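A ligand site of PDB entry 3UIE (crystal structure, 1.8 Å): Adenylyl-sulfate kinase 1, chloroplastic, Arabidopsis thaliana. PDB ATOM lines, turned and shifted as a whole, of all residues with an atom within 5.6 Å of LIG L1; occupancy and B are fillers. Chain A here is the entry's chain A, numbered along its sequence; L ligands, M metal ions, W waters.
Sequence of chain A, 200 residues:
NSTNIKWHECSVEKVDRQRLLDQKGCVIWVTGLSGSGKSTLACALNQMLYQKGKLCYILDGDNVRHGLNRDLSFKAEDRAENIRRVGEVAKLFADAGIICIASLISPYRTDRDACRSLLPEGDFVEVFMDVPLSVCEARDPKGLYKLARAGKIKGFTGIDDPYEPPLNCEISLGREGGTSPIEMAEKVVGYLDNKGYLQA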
ATOM      1  N   SER A  34       3.747  25.455 -22.492  1.00  0.00           N
ATOM      2  CA  SER A  34       3.786  26.601 -21.611  1.00  0.00           C
ATOM      3  C   SER A  34       2.385  27.204 -21.512  1.00  0.00           C
ATOM      4  O   SER A  34       1.712  27.399 -22.531  1.00  0.00           O
ATOM      5  CB  SER A  34       4.762  27.657 -22.139  1.00  0.00           C
ATOM      6  OG  SER A  34       4.967  28.678 -21.198  1.00  0.00           O
ATOM      7  N   LYS A  38       0.194  23.347 -15.952  1.00  0.00           N
ATOM      8  CA  LYS A  38       0.890  22.268 -15.245  1.00  0.00           C
ATOM      9  C   LYS A  38       1.173  22.608 -13.776  1.00  0.00           C
ATOM     10  O   LYS A  38       0.890  21.809 -12.877  1.00  0.00           O
ATOM     11  CB  LYS A  38       2.203  21.912 -15.969  1.00  0.00           C
ATOM     12  CG  LYS A  38       2.037  21.432 -17.410  1.00  0.00           C
ATOM     13  CD  LYS A  38       3.430  21.216 -18.026  1.00  0.00           C
ATOM     14  CE  LYS A  38       4.310  22.472 -17.974  1.00  0.00           C
ATOM     15  NZ  LYS A  38       3.841  23.537 -18.937  1.00  0.00           N
ATOM     16  N   GLY A  61       9.819  22.462 -13.492  1.00  0.00           N
ATOM     17  CA  GLY A  61      10.866  22.781 -14.448  1.00  0.00           C
ATOM     18  C   GLY A  61      11.526  24.116 -14.168  1.00  0.00           C
ATOM     19  O   GLY A  61      12.751  24.211 -14.165  1.00  0.00           O
ATOM     20  N   ASP A  62      10.732  25.142 -13.933  1.00  0.00           N
ATOM     21  CA  ASP A  62      11.317  26.452 -13.656  1.00  0.00           C
ATOM     22  C   ASP A  62      12.211  26.400 -12.411  1.00  0.00           C
ATOM     23  O   ASP A  62      13.383  26.795 -12.455  1.00  0.00           O
ATOM     24  CB  ASP A  62      10.227  27.517 -13.508  1.00  0.00           C
ATOM     25  CG  ASP A  62      10.791  28.930 -13.485  1.00  0.00           C
ATOM     26  OD1 ASP A  62      11.746  29.204 -14.250  1.00  0.00           O
ATOM     27  OD2 ASP A  62      10.283  29.768 -12.709  1.00  0.00           O
ATOM     28  N   ARG A  65      15.433  24.421 -12.812  1.00  0.00           N
ATOM     29  CA  ARG A  65      16.353  25.077 -13.746  1.00  0.00           C
ATOM     30  C   ARG A  65      17.151  26.187 -13.086  1.00  0.00           C
ATOM     31  O   ARG A  65      18.099  26.718 -13.674  1.00  0.00           O
ATOM     32  CB  ARG A  65      15.630  25.598 -14.989  1.00  0.00           C
ATOM     33  CG  ARG A  65      15.409  24.532 -16.064  1.00  0.00           C
ATOM     34  CD  ARG A  65      14.541  25.086 -17.191  1.00  0.00           C
ATOM     35  NE  ARG A  65      14.504  24.189 -18.356  1.00  0.00           N
ATOM     36  CZ  ARG A  65      15.507  24.080 -19.223  1.00  0.00           C
ATOM     37  NH1 ARG A  65      16.615  24.798 -19.050  1.00  0.00           N
ATOM     38  NH2 ARG A  65      15.414  23.246 -20.242  1.00  0.00           N
ATOM     39  N   PHE A  74      17.895  25.928 -23.382  1.00  0.00           N
ATOM     40  CA  PHE A  74      16.677  25.404 -23.988  1.00  0.00           C
ATOM     41  C   PHE A  74      16.917  24.816 -25.377  1.00  0.00           C
ATOM     42  O   PHE A  74      15.981  24.441 -26.065  1.00  0.00           O
ATOM     43  CB  PHE A  74      15.572  26.457 -24.016  1.00  0.00           C
ATOM     44  CG  PHE A  74      15.046  26.801 -22.656  1.00  0.00           C
ATOM     45  CD1 PHE A  74      13.976  26.114 -22.109  1.00  0.00           C
ATOM     46  CD2 PHE A  74      15.641  27.799 -21.904  1.00  0.00           C
ATOM     47  CE1 PHE A  74      13.503  26.436 -20.845  1.00  0.00           C
ATOM     48  CE2 PHE A  74      15.175  28.123 -20.648  1.00  0.00           C
ATOM     49  CZ  PHE A  74      14.107  27.447 -20.122  1.00  0.00           C
ATOM     50  N   ASP A  78      19.621  20.157 -24.477  1.00  0.00           N
ATOM     51  CA  ASP A  78      19.573  20.556 -23.078  1.00  0.00           C
ATOM     52  C   ASP A  78      18.194  20.302 -22.497  1.00  0.00           C
ATOM     53  O   ASP A  78      18.063  20.043 -21.297  1.00  0.00           O
ATOM     54  CB  ASP A  78      19.994  22.023 -22.904  1.00  0.00           C
ATOM     55  CG  ASP A  78      21.507  22.204 -22.848  1.00  0.00           C
ATOM     56  OD1 ASP A  78      22.244  21.256 -23.200  1.00  0.00           O
ATOM     57  OD2 ASP A  78      21.964  23.300 -22.449  1.00  0.00           O
ATOM     58  N   ARG A  79      17.157  20.371 -23.336  1.00  0.00           N
ATOM     59  CA  ARG A  79      15.820  19.965 -22.913  1.00  0.00           C
ATOM     60  C   ARG A  79      15.809  18.467 -22.583  1.00  0.00           C
ATOM     61  O   ARG A  79      15.234  18.042 -21.587  1.00  0.00           O
ATOM     62  CB  ARG A  79      14.765  20.265 -23.977  1.00  0.00           C
ATOM     63  CG  ARG A  79      14.418  21.745 -24.142  1.00  0.00           C
ATOM     64  CD  ARG A  79      13.194  21.889 -25.046  1.00  0.00           C
ATOM     65  NE  ARG A  79      13.050  23.224 -25.606  1.00  0.00           N
ATOM     66  CZ  ARG A  79      12.093  24.088 -25.261  1.00  0.00           C
ATOM     67  NH1 ARG A  79      11.208  23.771 -24.330  1.00  0.00           N
ATOM     68  NH2 ARG A  79      12.038  25.284 -25.855  1.00  0.00           N
ATOM     69  N   ASN A  82      17.632  18.033 -19.337  1.00  0.00           N
ATOM     70  CA  ASN A  82      16.757  18.551 -18.295  1.00  0.00           C
ATOM     71  C   ASN A  82      15.739  17.483 -17.885  1.00  0.00           C
ATOM     72  O   ASN A  82      15.569  17.180 -16.704  1.00  0.00           O
ATOM     73  CB  ASN A  82      16.019  19.791 -18.816  1.00  0.00           C
ATOM     74  CG  ASN A  82      15.118  20.427 -17.772  1.00  0.00           C
ATOM     75  OD1 ASN A  82      15.534  20.660 -16.638  1.00  0.00           O
ATOM     76  ND2 ASN A  82      13.884  20.705 -18.166  1.00  0.00           N
ATOM     77  N   ILE A  83      15.063  16.895 -18.874  1.00  0.00           N
ATOM     78  CA  ILE A  83      14.054  15.876 -18.656  1.00  0.00           C
ATOM     79  C   ILE A  83      14.694  14.633 -18.044  1.00  0.00           C
ATOM     80  O   ILE A  83      14.159  14.033 -17.107  1.00  0.00           O
ATOM     81  CB  ILE A  83      13.355  15.488 -19.990  1.00  0.00           C
ATOM     82  CG1 ILE A  83      12.564  16.679 -20.543  1.00  0.00           C
ATOM     83  CG2 ILE A  83      12.483  14.252 -19.817  1.00  0.00           C
ATOM     84  CD1 ILE A  83      12.214  16.550 -22.057  1.00  0.00           C
ATOM     85  N   SER A 103       6.534  18.718 -12.975  1.00  0.00           N
ATOM     86  CA  SER A 103       5.782  19.653 -13.799  1.00  0.00           C
ATOM     87  C   SER A 103       6.729  20.382 -14.742  1.00  0.00           C
ATOM     88  O   SER A 103       7.293  21.398 -14.371  1.00  0.00           O
ATOM     89  CB  SER A 103       5.040  20.652 -12.916  1.00  0.00           C
ATOM     90  OG  SER A 103       4.469  21.731 -13.653  1.00  0.00           O
ATOM     91  N   LEU A 104       6.929  19.840 -15.938  1.00  0.00           N
ATOM     92  CA  LEU A 104       7.895  20.353 -16.903  1.00  0.00           C
ATOM     93  C   LEU A 104       7.216  20.300 -18.254  1.00  0.00           C
ATOM     94  O   LEU A 104       6.432  19.387 -18.498  1.00  0.00           O
ATOM     95  CB  LEU A 104       9.102  19.421 -16.981  1.00  0.00           C
ATOM     96  CG  LEU A 104      10.416  19.510 -16.225  1.00  0.00           C
ATOM     97  CD1 LEU A 104      10.240  19.241 -14.746  1.00  0.00           C
ATOM     98  CD2 LEU A 104      11.369  18.492 -16.846  1.00  0.00           C
ATOM     99  N   ILE A 105       7.516  21.252 -19.133  1.00  0.00           N
ATOM    100  CA  ILE A 105       6.977  21.183 -20.493  1.00  0.00           C
ATOM    101  C   ILE A 105       7.277  19.819 -21.106  1.00  0.00           C
ATOM    102  O   ILE A 105       6.397  19.186 -21.691  1.00  0.00           O
ATOM    103  CB  ILE A 105       7.528  22.315 -21.404  1.00  0.00           C
ATOM    104  CG1 ILE A 105       7.082  23.674 -20.874  1.00  0.00           C
ATOM    105  CG2 ILE A 105       7.055  22.122 -22.853  1.00  0.00           C
ATOM    106  CD1 ILE A 105       7.653  24.863 -21.659  1.00  0.00           C
ATOM    107  N   SER A 106       8.518  19.368 -20.932  1.00  0.00           N
ATOM    108  CA  SER A 106       8.978  18.044 -21.413  1.00  0.00           C
ATOM    109  C   SER A 106       8.392  17.674 -22.770  1.00  0.00           C
ATOM    110  O   SER A 106       7.622  16.720 -22.880  1.00  0.00           O
ATOM    111  CB  SER A 106       8.721  16.955 -20.366  1.00  0.00           C
ATOM    112  OG  SER A 106       7.411  17.020 -19.833  1.00  0.00           O
ATOM    113  N   PRO A 107       8.754  18.429 -23.816  1.00  0.00           N
ATOM    114  CA  PRO A 107       8.056  18.357 -25.109  1.00  0.00           C
ATOM    115  C   PRO A 107       8.305  17.085 -25.909  1.00  0.00           C
ATOM    116  O   PRO A 107       7.483  16.762 -26.754  1.00  0.00           O
ATOM    117  CB  PRO A 107       8.609  19.582 -25.857  1.00  0.00           C
ATOM    118  CG  PRO A 107       9.981  19.779 -25.275  1.00  0.00           C
ATOM    119  CD  PRO A 107       9.838  19.427 -23.819  1.00  0.00           C
ATOM    120  N   LYS A 142       3.096  34.941 -18.649  1.00  0.00           N
ATOM    121  CA  LYS A 142       4.425  35.511 -18.497  1.00  0.00           C
ATOM    122  C   LYS A 142       4.863  36.317 -19.719  1.00  0.00           C
ATOM    123  O   LYS A 142       5.975  36.850 -19.744  1.00  0.00           O
ATOM    124  CB  LYS A 142       5.446  34.404 -18.209  1.00  0.00           C
ATOM    125  CG  LYS A 142       5.073  33.505 -17.041  1.00  0.00           C
ATOM    126  CD  LYS A 142       5.985  32.280 -16.971  1.00  0.00           C
ATOM    127  CE  LYS A 142       5.410  31.224 -16.031  1.00  0.00           C
ATOM    128  NZ  LYS A 142       6.277  30.005 -15.944  1.00  0.00           N
ATOM    129  N   LEU A 144       5.501  35.155 -22.643  1.00  0.00           N
ATOM    130  CA  LEU A 144       6.510  34.412 -23.389  1.00  0.00           C
ATOM    131  C   LEU A 144       6.129  34.166 -24.844  1.00  0.00           C
ATOM    132  O   LEU A 144       6.990  34.231 -25.723  1.00  0.00           O
ATOM    133  CB  LEU A 144       6.805  33.074 -22.718  1.00  0.00           C
ATOM    134  CG  LEU A 144       7.491  33.171 -21.361  1.00  0.00           C
ATOM    135  CD1 LEU A 144       7.562  31.800 -20.739  1.00  0.00           C
ATOM    136  CD2 LEU A 144       8.860  33.783 -21.509  1.00  0.00           C
ATOM    137  N   ILE A 153      12.505  35.474 -28.338  1.00  0.00           N
ATOM    138  CA  ILE A 153      12.850  34.156 -27.834  1.00  0.00           C
ATOM    139  C   ILE A 153      12.832  33.181 -28.993  1.00  0.00           C
ATOM    140  O   ILE A 153      11.801  33.006 -29.633  1.00  0.00           O
ATOM    141  CB  ILE A 153      11.853  33.693 -26.746  1.00  0.00           C
ATOM    142  CG1 ILE A 153      11.862  34.653 -25.558  1.00  0.00           C
ATOM    143  CG2 ILE A 153      12.179  32.263 -26.290  1.00  0.00           C
ATOM    144  CD1 ILE A 153      10.934  34.234 -24.440  1.00  0.00           C
ATOM    145  N   LYS A 154      13.963  32.565 -29.279  1.00  0.00           N
ATOM    146  CA  LYS A 154      14.077  31.612 -30.376  1.00  0.00           C
ATOM    147  C   LYS A 154      13.747  30.204 -29.898  1.00  0.00           C
ATOM    148  O   LYS A 154      13.950  29.880 -28.734  1.00  0.00           O
ATOM    149  CB  LYS A 154      15.481  31.654 -30.973  1.00  0.00           C
ATOM    150  CG  LYS A 154      15.736  30.675 -32.107  1.00  0.00           C
ATOM    151  CD  LYS A 154      17.177  30.759 -32.607  1.00  0.00           C
ATOM    152  CE  LYS A 154      17.403  29.835 -33.789  1.00  0.00           C
ATOM    153  NZ  LYS A 154      18.795  29.945 -34.321  1.00  0.00           N
ATOM    154  N   GLY A 155      13.221  29.370 -30.796  1.00  0.00           N
ATOM    155  CA  GLY A 155      12.990  27.967 -30.488  1.00  0.00           C
ATOM    156  C   GLY A 155      12.014  27.690 -29.366  1.00  0.00           C
ATOM    157  O   GLY A 155      12.147  26.686 -28.650  1.00  0.00           O
ATOM    158  N   PHE A 156      11.019  28.544 -29.203  1.00  0.00           N
ATOM    159  CA  PHE A 156      10.035  28.371 -28.138  1.00  0.00           C
ATOM    160  C   PHE A 156       9.039  27.250 -28.445  1.00  0.00           C
ATOM    161  O   PHE A 156       8.484  27.192 -29.549  1.00  0.00           O
ATOM    162  CB  PHE A 156       9.279  29.684 -27.878  1.00  0.00           C
ATOM    163  CG  PHE A 156       8.506  29.682 -26.587  1.00  0.00           C
ATOM    164  CD1 PHE A 156       9.176  29.778 -25.377  1.00  0.00           C
ATOM    165  CD2 PHE A 156       7.129  29.599 -26.580  1.00  0.00           C
ATOM    166  CE1 PHE A 156       8.481  29.794 -24.176  1.00  0.00           C
ATOM    167  CE2 PHE A 156       6.423  29.601 -25.392  1.00  0.00           C
ATOM    168  CZ  PHE A 156       7.099  29.699 -24.190  1.00  0.00           C
ATOM    169  N   THR A 157       8.816  26.375 -27.479  1.00  0.00           N
ATOM    170  CA  THR A 157       7.907  25.249 -27.636  1.00  0.00           C
ATOM    171  C   THR A 157       6.514  25.645 -28.126  1.00  0.00           C
ATOM    172  O   THR A 157       5.861  26.500 -27.531  1.00  0.00           O
ATOM    173  CB  THR A 157       7.783  24.463 -26.308  1.00  0.00           C
ATOM    174  OG1 THR A 157       9.058  23.946 -25.952  1.00  0.00           O
ATOM    175  CG2 THR A 157       6.804  23.303 -26.453  1.00  0.00           C
HETATM  176  S1  LIG L   1      11.564  21.804 -20.799  1.00  0.00           S
HETATM  177  O1  LIG L   1      12.987  21.710 -20.674  1.00  0.00           O
HETATM  178  O2  LIG L   1      11.208  21.797 -22.228  1.00  0.00           O
HETATM  179  O3  LIG L   1      10.885  20.665 -20.142  1.00  0.00           O
HETATM  180  P1  LIG L   1      10.901  23.479 -18.675  1.00  0.00           P
HETATM  181  O4  LIG L   1      12.041  22.918 -17.871  1.00  0.00           O
HETATM  182  O5  LIG L   1       9.546  23.086 -18.102  1.00  0.00           O
HETATM  183  O6  LIG L   1      11.057  23.109 -20.215  1.00  0.00           O
HETATM  184  O7  LIG L   1      11.040  25.045 -18.638  1.00  0.00           O
HETATM  185  C1  LIG L   1       9.977  25.846 -19.079  1.00  0.00           C
HETATM  186  C2  LIG L   1       9.941  27.185 -18.548  1.00  0.00           C
HETATM  187  O8  LIG L   1      11.074  27.903 -19.008  1.00  0.00           O
HETATM  188  C3  LIG L   1       8.731  27.875 -19.065  1.00  0.00           C
HETATM  189  O9  LIG L   1       7.981  28.319 -17.981  1.00  0.00           O
HETATM  190  C4  LIG L   1       9.181  29.022 -19.735  1.00  0.00           C
HETATM  191  O10 LIG L   1       8.775  30.093 -18.952  1.00  0.00           O
HETATM  192  C5  LIG L   1      10.663  29.024 -19.720  1.00  0.00           C
HETATM  193  N1  LIG L   1      11.214  29.120 -21.046  1.00  0.00           N
HETATM  194  C6  LIG L   1      12.233  29.925 -21.427  1.00  0.00           C
HETATM  195  N2  LIG L   1      12.522  29.678 -22.715  1.00  0.00           N
HETATM  196  C7  LIG L   1      11.700  28.704 -23.154  1.00  0.00           C
HETATM  197  C8  LIG L   1      11.525  28.047 -24.388  1.00  0.00           C
HETATM  198  N3  LIG L   1      12.358  28.371 -25.493  1.00  0.00           N
HETATM  199  N4  LIG L   1      10.560  27.092 -24.514  1.00  0.00           N
HETATM  200  C9  LIG L   1       9.779  26.776 -23.469  1.00  0.00           C
HETATM  201  N5  LIG L   1       9.921  27.391 -22.275  1.00  0.00           N
HETATM  202  C10 LIG L   1      10.859  28.347 -22.091  1.00  0.00           C
HETATM  203  P1  LG2 L   2       4.922  26.916 -17.804  1.00  0.00           P
HETATM  204  O1  LG2 L   2       5.528  28.140 -18.654  1.00  0.00           O
HETATM  205  O2  LG2 L   2       5.557  27.039 -16.415  1.00  0.00           O
HETATM  206  O3  LG2 L   2       5.273  25.613 -18.462  1.00  0.00           O
HETATM  207  P2  LG2 L   2       2.288  26.022 -16.869  1.00  0.00           P
HETATM  208  O4  LG2 L   2       2.796  25.783 -15.400  1.00  0.00           O
HETATM  209  O5  LG2 L   2       1.860  24.797 -17.710  1.00  0.00           O
HETATM  210  N1  LG2 L   2       3.273  27.212 -17.589  1.00  0.00           N
HETATM  211  P3  LG2 L   2       0.549  27.650 -15.184  1.00  0.00           P
HETATM  212  O6  LG2 L   2       1.561  28.646 -14.714  1.00  0.00           O
HETATM  213  O7  LG2 L   2       0.176  26.638 -14.143  1.00  0.00           O
HETATM  214  O8  LG2 L   2       1.069  27.040 -16.535  1.00  0.00           O
HETATM  215  O9  LG2 L   2      -0.768  28.378 -15.658  1.00  0.00           O
HETATM  216  C1  LG2 L   2      -0.765  29.400 -16.603  1.00  0.00           C
HETATM  217  C2  LG2 L   2      -1.850  30.310 -16.483  1.00  0.00           C
HETATM  218  O10 LG2 L   2      -3.113  29.648 -16.795  1.00  0.00           O
HETATM  219  C3  LG2 L   2      -1.908  30.737 -15.084  1.00  0.00           C
HETATM  220  O11 LG2 L   2      -1.962  32.152 -15.012  1.00  0.00           O
HETATM  221  C4  LG2 L   2      -3.122  30.148 -14.520  1.00  0.00           C
HETATM  222  O12 LG2 L   2      -3.854  31.090 -13.779  1.00  0.00           O
HETATM  223  C5  LG2 L   2      -3.937  29.718 -15.684  1.00  0.00           C
HETATM  224  N2  LG2 L   2      -4.585  28.439 -15.390  1.00  0.00           N
HETATM  225  C6  LG2 L   2      -3.954  27.394 -14.821  1.00  0.00           C
HETATM  226  N3  LG2 L   2      -4.840  26.408 -14.703  1.00  0.00           N
HETATM  227  C7  LG2 L   2      -6.025  26.832 -15.185  1.00  0.00           C
HETATM  228  C8  LG2 L   2      -7.270  26.225 -15.293  1.00  0.00           C
HETATM  229  N4  LG2 L   2      -7.450  24.857 -14.824  1.00  0.00           N
HETATM  230  N5  LG2 L   2      -8.275  26.921 -15.837  1.00  0.00           N
HETATM  231  C9  LG2 L   2      -8.088  28.185 -16.263  1.00  0.00           C
HETATM  232  N6  LG2 L   2      -6.919  28.798 -16.165  1.00  0.00           N
HETATM  233  C10 LG2 L   2      -5.861  28.141 -15.631  1.00  0.00           C
HETATM  234 MG    MG M   1       4.812  26.204 -14.670  1.00  0.00          MG
HETATM  235  O   HOH W   1       7.253  24.339 -16.989  1.00  0.00           O
HETATM  236  O   HOH W   2      13.054  28.591 -16.455  1.00  0.00           O
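An oxygen (O9) of LIG L1 is in hydrogen-bond range of an oxygen (O1) of LG2 L2 (2.5 Å).
Water W1 bridges an oxygen (O3) of LG2 L2 (2.8 Å) and an oxygen (O5) of LIG L1 (2.8 Å). Water W2 bridges OD1 of Asp 62 and O8 of LIG L1.
O of Ser 103 lies within hydrogen-bond range of N of Gly 61. The side-chain hydroxyl (OG1) of Thr 157 sits at hydrogen-bond distance from the guanidinium group (NH1) of Arg 79, 2.7 Å away. NH2 of Arg 79 is in hydrogen-bond range of O of Gly 155, at 3.1 Å. The guanidinium group of Arg 79 is in hydrogen-bond range of the backbone carbonyl oxygen of Phe 74 (3.2 Å). O of Leu 104 lies within hydrogen-bond range of OG of Ser 106, 2.9 Å away.
CA of Gly 61 touches O4 of LIG L1, at 3.6 Å. Phe 74 touches LIG L1. Leu 104 touches LIG L1. Pro 107 touches LIG L1 (CD to O2, 3.2 Å). Leu 144 touches LIG L1. Ile 153 touches LIG L1. Lys 154 touches LIG L1 (O to N3, 3.9 Å). Gly 155 touches LIG L1 (O to N3, 3.6 Å). Phe 156 touches LIG L1 (CD1 to C8, 3.1 Å). Thr 157 touches LIG L1. Hydrophobic or aromatic side chains within 4 Å of LIG L1: Phe 74, Leu 104, Ile 105, Pro 107, Leu 144, Ile 153 and Phe 156. Within 4 Å of LIG L1: Gly 61, Arg 65, Phe 74, Arg 79, Asn 82, Leu 104, Ile 105, Ser 106, Pro 107, Lys 142, Leu 144, Ile 153, Lys 154, Gly 155, Phe 156 and Thr 157. The nearest printed residue that does not touch LIG L1 is Ile 83 (4.3 Å).
O9 of LIG L1 sits at hydrogen-bond distance from NZ of Lys 142. O3 of LG2 L2 lies within salt-bridge range of NZ of Lys 38. ND2 of Asn 82 sits at hydrogen-bond distance from O1 of LIG L1, 2.8 Å away. The backbone NH of Ser 106 is in hydrogen-bond range of an oxygen (O3) of LIG L1 (2.8 Å). An oxygen (O1) of LG2 L2 lies within hydrogen-bond range of the side-chain hydroxyl of Ser 34 (2.7 Å). The side-chain amino group (NZ) of Lys 142 lies within salt-bridge range of an oxygen (O1) of LG2 L2, at 3.4 Å. The guanidinium group (NE) of Arg 65 lies within salt-bridge range of an oxygen (O4) of LIG L1, at 2.8 Å. NH1 of Arg 79 is in salt-bridge range of O2 of LIG L1 (2.9 Å). N of Ile 105 is in hydrogen-bond range of O5 of LIG L1 (2.9 Å). O5 of LG2 L2 lies within hydrogen-bond range of N of Lys 38, 2.8 Å away.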
